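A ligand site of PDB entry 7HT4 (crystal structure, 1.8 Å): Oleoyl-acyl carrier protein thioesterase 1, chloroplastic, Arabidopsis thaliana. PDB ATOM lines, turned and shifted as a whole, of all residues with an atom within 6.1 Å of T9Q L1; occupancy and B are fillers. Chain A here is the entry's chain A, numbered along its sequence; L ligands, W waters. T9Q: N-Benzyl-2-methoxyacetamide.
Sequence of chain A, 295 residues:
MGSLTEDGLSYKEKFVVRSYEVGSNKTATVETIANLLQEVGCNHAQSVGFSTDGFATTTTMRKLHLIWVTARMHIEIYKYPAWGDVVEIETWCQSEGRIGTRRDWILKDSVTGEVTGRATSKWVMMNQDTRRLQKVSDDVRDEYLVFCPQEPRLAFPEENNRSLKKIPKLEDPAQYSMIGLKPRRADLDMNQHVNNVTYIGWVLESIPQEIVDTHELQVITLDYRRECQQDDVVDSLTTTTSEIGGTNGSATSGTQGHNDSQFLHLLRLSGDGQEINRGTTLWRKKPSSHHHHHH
The side-chain sulfur of Cys 148 sits at hydrogen-bond distance from the backbone carbonyl oxygen of Cys 93 (3.2 Å).
The guanidinium group of Arg 103 lies within hydrogen-bond range of a ring nitrogen (ND1) of His 44, 3.0 Å away.
The backbone NH (N) of Trp 123 lies within hydrogen-bond range of the backbone carbonyl oxygen (O) of Thr 101 (3.0 Å).
The backbone carbonyl oxygen (O) of Ala 56 sits at hydrogen-bond distance from the indole nitrogen (NE1) of Trp 68, at 3.3 Å.
The backbone carbonyl oxygen (O) of Arg 102 sits close to the side-chain sulfur (SG) of Cys 93, 3.5 Å away.
The backbone carbonyl oxygen of Ala 45 sits at hydrogen-bond distance from the backbone NH of Phe 50.
Residues that only touch T9Q L1: His 44, Ala 45, Val 48, Phe 50, Phe 55, Ala 56, Trp 68, Cys 93 and Phe 147.
Hydrophobic or aromatic side chains that line T9Q L1: His 44, Val 48, Phe 50, Phe 55, Ala 56, Trp 68 and Phe 147.
Within 4 Å of T9Q L1: His 44, Ala 45, Val 48, Phe 50, Phe 55, Ala 56, Trp 68, Cys 93, Thr 101, Arg 103 and Phe 147.
NH1 of Arg 103 lies within hydrogen-bond range of O05 of T9Q L1, at 2.7 Å.
An oxygen (O02) of T9Q L1 is in hydrogen-bond range of the side-chain hydroxyl of Thr 101, at 2.6 Å.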
ATOM      1  N   GLY A  41      23.725  10.097  25.627  1.00  0.00           N
ATOM      2  CA  GLY A  41      22.428  10.105  24.950  1.00  0.00           C
ATOM      3  C   GLY A  41      21.591   8.915  25.383  1.00  0.00           C
ATOM      4  O   GLY A  41      20.400   9.054  25.674  1.00  0.00           O
ATOM      5  N   HIS A  44      20.479   9.277  29.108  1.00  0.00           N
ATOM      6  CA  HIS A  44      19.388  10.234  29.222  1.00  0.00           C
ATOM      7  C   HIS A  44      18.054   9.544  28.860  1.00  0.00           C
ATOM      8  O   HIS A  44      17.102   9.661  29.637  1.00  0.00           O
ATOM      9  CB  HIS A  44      19.618  11.478  28.342  1.00  0.00           C
ATOM     10  CG  HIS A  44      18.601  12.562  28.517  1.00  0.00           C
ATOM     11  ND1 HIS A  44      18.558  13.643  27.649  1.00  0.00           N
ATOM     12  CD2 HIS A  44      17.623  12.715  29.451  1.00  0.00           C
ATOM     13  CE1 HIS A  44      17.563  14.401  28.069  1.00  0.00           C
ATOM     14  NE2 HIS A  44      16.957  13.872  29.142  1.00  0.00           N
ATOM     15  N   ALA A  45      17.997   8.771  27.744  1.00  0.00           N
ATOM     16  CA  ALA A  45      16.762   8.065  27.354  1.00  0.00           C
ATOM     17  C   ALA A  45      16.338   7.049  28.427  1.00  0.00           C
ATOM     18  O   ALA A  45      15.145   6.922  28.723  1.00  0.00           O
ATOM     19  CB  ALA A  45      16.967   7.359  26.013  1.00  0.00           C
ATOM     20  N   VAL A  48      14.547   8.368  31.714  1.00  0.00           N
ATOM     21  CA  VAL A  48      13.135   8.761  31.632  1.00  0.00           C
ATOM     22  C   VAL A  48      12.222   7.659  31.037  1.00  0.00           C
ATOM     23  O   VAL A  48      11.118   7.954  30.570  1.00  0.00           O
ATOM     24  CB  VAL A  48      12.934  10.118  30.930  1.00  0.00           C
ATOM     25  CG1 VAL A  48      13.492  11.254  31.785  1.00  0.00           C
ATOM     26  CG2 VAL A  48      13.550  10.121  29.552  1.00  0.00           C
ATOM     27  N   PHE A  50      12.676   5.376  28.398  1.00  0.00           N
ATOM     28  CA  PHE A  50      12.731   4.913  27.015  1.00  0.00           C
ATOM     29  C   PHE A  50      13.312   3.501  26.910  1.00  0.00           C
ATOM     30  O   PHE A  50      14.081   3.078  27.777  1.00  0.00           O
ATOM     31  CB  PHE A  50      13.423   5.918  26.100  1.00  0.00           C
ATOM     32  CG  PHE A  50      12.560   7.111  25.806  1.00  0.00           C
ATOM     33  CD1 PHE A  50      11.454   7.004  24.987  1.00  0.00           C
ATOM     34  CD2 PHE A  50      12.868   8.358  26.319  1.00  0.00           C
ATOM     35  CE1 PHE A  50      10.687   8.109  24.677  1.00  0.00           C
ATOM     36  CE2 PHE A  50      12.079   9.459  26.028  1.00  0.00           C
ATOM     37  CZ  PHE A  50      11.003   9.331  25.207  1.00  0.00           C
ATOM     38  N   PHE A  55      16.815   2.377  20.818  1.00  0.00           N
ATOM     39  CA  PHE A  55      17.043   3.740  21.280  1.00  0.00           C
ATOM     40  C   PHE A  55      15.842   4.674  21.043  1.00  0.00           C
ATOM     41  O   PHE A  55      15.299   4.736  19.931  1.00  0.00           O
ATOM     42  CB  PHE A  55      18.353   4.329  20.709  1.00  0.00           C
ATOM     43  CG  PHE A  55      18.607   5.768  21.110  1.00  0.00           C
ATOM     44  CD1 PHE A  55      18.411   6.802  20.212  1.00  0.00           C
ATOM     45  CD2 PHE A  55      19.004   6.088  22.406  1.00  0.00           C
ATOM     46  CE1 PHE A  55      18.606   8.121  20.599  1.00  0.00           C
ATOM     47  CE2 PHE A  55      19.189   7.408  22.782  1.00  0.00           C
ATOM     48  CZ  PHE A  55      19.017   8.415  21.877  1.00  0.00           C
ATOM     49  N   ALA A  56      15.415   5.355  22.119  1.00  0.00           N
ATOM     50  CA  ALA A  56      14.342   6.349  22.154  1.00  0.00           C
ATOM     51  C   ALA A  56      12.953   5.852  21.711  1.00  0.00           C
ATOM     52  O   ALA A  56      12.088   6.683  21.434  1.00  0.00           O
ATOM     53  CB  ALA A  56      14.746   7.582  21.343  1.00  0.00           C
ATOM     54  N   TRP A  68      14.031   5.313  15.630  1.00  0.00           N
ATOM     55  CA  TRP A  68      14.634   6.606  15.366  1.00  0.00           C
ATOM     56  C   TRP A  68      16.007   6.322  14.781  1.00  0.00           C
ATOM     57  O   TRP A  68      16.742   5.466  15.301  1.00  0.00           O
ATOM     58  CB  TRP A  68      14.831   7.399  16.657  1.00  0.00           C
ATOM     59  CG  TRP A  68      13.563   7.932  17.226  1.00  0.00           C
ATOM     60  CD1 TRP A  68      12.890   7.457  18.313  1.00  0.00           C
ATOM     61  CD2 TRP A  68      12.793   9.035  16.732  1.00  0.00           C
ATOM     62  NE1 TRP A  68      11.795   8.238  18.567  1.00  0.00           N
ATOM     63  CE2 TRP A  68      11.699   9.199  17.601  1.00  0.00           C
ATOM     64  CE3 TRP A  68      12.958   9.931  15.666  1.00  0.00           C
ATOM     65  CZ2 TRP A  68      10.764  10.217  17.433  1.00  0.00           C
ATOM     66  CZ3 TRP A  68      12.032  10.948  15.508  1.00  0.00           C
ATOM     67  CH2 TRP A  68      10.949  11.082  16.383  1.00  0.00           C
ATOM     68  N   TRP A  92      20.528  17.331  25.763  1.00  0.00           N
ATOM     69  CA  TRP A  92      19.116  17.579  25.802  1.00  0.00           C
ATOM     70  C   TRP A  92      18.528  17.325  24.413  1.00  0.00           C
ATOM     71  O   TRP A  92      19.263  17.282  23.413  1.00  0.00           O
ATOM     72  CB  TRP A  92      18.828  19.013  26.310  1.00  0.00           C
ATOM     73  CG  TRP A  92      19.283  20.105  25.377  1.00  0.00           C
ATOM     74  CD1 TRP A  92      18.538  20.731  24.425  1.00  0.00           C
ATOM     75  CD2 TRP A  92      20.575  20.716  25.346  1.00  0.00           C
ATOM     76  NE1 TRP A  92      19.305  21.648  23.756  1.00  0.00           N
ATOM     77  CE2 TRP A  92      20.535  21.707  24.342  1.00  0.00           C
ATOM     78  CE3 TRP A  92      21.745  20.553  26.077  1.00  0.00           C
ATOM     79  CZ2 TRP A  92      21.631  22.521  24.060  1.00  0.00           C
ATOM     80  CZ3 TRP A  92      22.828  21.373  25.798  1.00  0.00           C
ATOM     81  CH2 TRP A  92      22.775  22.318  24.770  1.00  0.00           C
ATOM     82  N   CYS A  93      17.221  17.127  24.345  1.00  0.00           N
ATOM     83  CA  CYS A  93      16.535  16.876  23.088  1.00  0.00           C
ATOM     84  C   CYS A  93      15.435  17.917  22.864  1.00  0.00           C
ATOM     85  O   CYS A  93      14.868  18.416  23.824  1.00  0.00           O
ATOM     86  CB  CYS A  93      15.972  15.452  23.087  1.00  0.00           C
ATOM     87  SG  CYS A  93      15.139  14.985  21.550  1.00  0.00           S
ATOM     88  N   THR A 101      13.466  15.006  15.402  1.00  0.00           N
ATOM     89  CA  THR A 101      13.974  15.614  16.623  1.00  0.00           C
ATOM     90  C   THR A 101      15.456  16.046  16.450  1.00  0.00           C
ATOM     91  O   THR A 101      16.126  15.649  15.489  1.00  0.00           O
ATOM     92  CB  THR A 101      13.840  14.618  17.838  1.00  0.00           C
ATOM     93  OG1 THR A 101      14.870  13.639  17.758  1.00  0.00           O
ATOM     94  CG2 THR A 101      12.512  13.916  17.888  1.00  0.00           C
ATOM     95  N   ARG A 102      15.968  16.801  17.420  1.00  0.00           N
ATOM     96  CA  ARG A 102      17.336  17.250  17.455  1.00  0.00           C
ATOM     97  C   ARG A 102      17.903  16.957  18.847  1.00  0.00           C
ATOM     98  O   ARG A 102      17.233  17.246  19.848  1.00  0.00           O
ATOM     99  CB  ARG A 102      17.396  18.753  17.189  1.00  0.00           C
ATOM    100  CG  ARG A 102      18.781  19.226  16.783  1.00  0.00           C
ATOM    101  CD  ARG A 102      18.868  20.720  16.725  1.00  0.00           C
ATOM    102  NE  ARG A 102      18.929  21.263  18.071  1.00  0.00           N
ATOM    103  CZ  ARG A 102      17.950  21.947  18.659  1.00  0.00           C
ATOM    104  NH1 ARG A 102      18.091  22.397  19.894  1.00  0.00           N
ATOM    105  NH2 ARG A 102      16.841  22.230  17.989  1.00  0.00           N
ATOM    106  N   ARG A 103      19.070  16.301  18.938  1.00  0.00           N
ATOM    107  CA  ARG A 103      19.700  16.104  20.238  1.00  0.00           C
ATOM    108  C   ARG A 103      20.995  16.914  20.189  1.00  0.00           C
ATOM    109  O   ARG A 103      21.728  16.792  19.187  1.00  0.00           O
ATOM    110  CB  ARG A 103      19.996  14.619  20.554  1.00  0.00           C
ATOM    111  CG  ARG A 103      20.790  14.494  21.870  1.00  0.00           C
ATOM    112  CD  ARG A 103      20.900  13.074  22.400  1.00  0.00           C
ATOM    113  NE  ARG A 103      19.645  12.585  22.976  1.00  0.00           N
ATOM    114  CZ  ARG A 103      19.266  12.800  24.238  1.00  0.00           C
ATOM    115  NH1 ARG A 103      18.119  12.306  24.692  1.00  0.00           N
ATOM    116  NH2 ARG A 103      20.033  13.500  25.057  1.00  0.00           N
ATOM    117  N   TRP A 123      17.553  13.514  14.025  1.00  0.00           N
ATOM    118  CA  TRP A 123      16.978  12.179  14.012  1.00  0.00           C
ATOM    119  C   TRP A 123      15.665  12.169  13.238  1.00  0.00           C
ATOM    120  O   TRP A 123      14.880  13.101  13.354  1.00  0.00           O
ATOM    121  CB  TRP A 123      16.692  11.708  15.450  1.00  0.00           C
ATOM    122  CG  TRP A 123      17.915  11.638  16.303  1.00  0.00           C
ATOM    123  CD1 TRP A 123      18.538  12.675  16.925  1.00  0.00           C
ATOM    124  CD2 TRP A 123      18.644  10.464  16.677  1.00  0.00           C
ATOM    125  NE1 TRP A 123      19.655  12.228  17.587  1.00  0.00           N
ATOM    126  CE2 TRP A 123      19.724  10.868  17.483  1.00  0.00           C
ATOM    127  CE3 TRP A 123      18.484   9.092  16.424  1.00  0.00           C
ATOM    128  CZ2 TRP A 123      20.634   9.971  18.038  1.00  0.00           C
ATOM    129  CZ3 TRP A 123      19.426   8.208  16.912  1.00  0.00           C
ATOM    130  CH2 TRP A 123      20.477   8.647  17.722  1.00  0.00           C
ATOM    131  N   TYR A 144       7.333  12.160  23.931  1.00  0.00           N
ATOM    132  CA  TYR A 144       8.665  12.677  24.256  1.00  0.00           C
ATOM    133  C   TYR A 144       8.718  14.185  24.584  1.00  0.00           C
ATOM    134  O   TYR A 144       9.667  14.609  25.233  1.00  0.00           O
ATOM    135  CB  TYR A 144       9.698  12.308  23.174  1.00  0.00           C
ATOM    136  CG  TYR A 144       9.600  13.112  21.890  1.00  0.00           C
ATOM    137  CD1 TYR A 144      10.253  14.329  21.770  1.00  0.00           C
ATOM    138  CD2 TYR A 144       9.010  12.573  20.757  1.00  0.00           C
ATOM    139  CE1 TYR A 144      10.228  15.045  20.579  1.00  0.00           C
ATOM    140  CE2 TYR A 144       8.992  13.276  19.556  1.00  0.00           C
ATOM    141  CZ  TYR A 144       9.587  14.523  19.468  1.00  0.00           C
ATOM    142  OH  TYR A 144       9.561  15.240  18.306  1.00  0.00           O
ATOM    143  N   PHE A 147       9.715  15.686  28.052  1.00  0.00           N
ATOM    144  CA  PHE A 147      11.106  15.555  28.464  1.00  0.00           C
ATOM    145  C   PHE A 147      12.052  16.573  27.771  1.00  0.00           C
ATOM    146  O   PHE A 147      13.253  16.516  28.003  1.00  0.00           O
ATOM    147  CB  PHE A 147      11.612  14.113  28.209  1.00  0.00           C
ATOM    148  CG  PHE A 147      10.714  13.054  28.781  1.00  0.00           C
ATOM    149  CD1 PHE A 147      10.500  12.978  30.151  1.00  0.00           C
ATOM    150  CD2 PHE A 147      10.027  12.184  27.956  1.00  0.00           C
ATOM    151  CE1 PHE A 147       9.611  12.051  30.669  1.00  0.00           C
ATOM    152  CE2 PHE A 147       9.182  11.227  28.486  1.00  0.00           C
ATOM    153  CZ  PHE A 147       8.965  11.168  29.842  1.00  0.00           C
ATOM    154  N   CYS A 148      11.496  17.520  27.001  1.00  0.00           N
ATOM    155  CA  CYS A 148      12.198  18.525  26.203  1.00  0.00           C
ATOM    156  C   CYS A 148      11.852  19.932  26.702  1.00  0.00           C
ATOM    157  O   CYS A 148      10.675  20.210  26.946  1.00  0.00           O
ATOM    158  CB  CYS A 148      11.777  18.402  24.739  1.00  0.00           C
ATOM    159  SG  CYS A 148      12.145  16.801  23.970  1.00  0.00           S
HETATM  160  C10 T9Q L   1      15.394  12.044  26.667  1.00  0.00           C
HETATM  161  C13 T9Q L   1      13.978  12.676  24.391  1.00  0.00           C
HETATM  162  C01 T9Q L   1      14.997  10.400  18.877  1.00  0.00           C
HETATM  163  C03 T9Q L   1      16.452  11.742  20.236  1.00  0.00           C
HETATM  164  C04 T9Q L   1      16.213  11.262  21.648  1.00  0.00           C
HETATM  165  C07 T9Q L   1      14.567  10.474  23.311  1.00  0.00           C
HETATM  166  C08 T9Q L   1      14.616  11.449  24.460  1.00  0.00           C
HETATM  167  C09 T9Q L   1      15.287  11.126  25.631  1.00  0.00           C
HETATM  168  C11 T9Q L   1      14.747  13.245  26.582  1.00  0.00           C
HETATM  169  C12 T9Q L   1      14.032  13.560  25.451  1.00  0.00           C
HETATM  170  N06 T9Q L   1      14.949  11.035  22.013  1.00  0.00           N
HETATM  171  O02 T9Q L   1      15.288  11.664  19.448  1.00  0.00           O
HETATM  172  O05 T9Q L   1      17.178  11.135  22.402  1.00  0.00           O
HETATM  173  C10 T9Q L   2      25.736   9.708  15.530  1.00  0.00           C
HETATM  174  C13 T9Q L   2      26.826   9.616  18.049  1.00  0.00           C
HETATM  175  C01 T9Q L   2      22.125   5.331  20.215  1.00  0.00           C
HETATM  176  C03 T9Q L   2      22.411   7.570  20.960  1.00  0.00           C
HETATM  177  C04 T9Q L   2      22.988   8.913  20.542  1.00  0.00           C
HETATM  178  C07 T9Q L   2      24.599  10.066  19.122  1.00  0.00           C
HETATM  179  C08 T9Q L   2      25.462   9.819  17.908  1.00  0.00           C
HETATM  180  C09 T9Q L   2      24.930   9.897  16.632  1.00  0.00           C
HETATM  181  C11 T9Q L   2      27.092   9.503  15.678  1.00  0.00           C
HETATM  182  C12 T9Q L   2      27.629   9.444  16.933  1.00  0.00           C
HETATM  183  N06 T9Q L   2      23.873   8.883  19.559  1.00  0.00           N
HETATM  184  O02 T9Q L   2      22.743   6.602  19.992  1.00  0.00           O
HETATM  185  O05 T9Q L   2      22.639   9.937  21.125  1.00  0.00           O
HETATM  186  O   HOH W   1      12.160  11.000  20.959  1.00  0.00           O
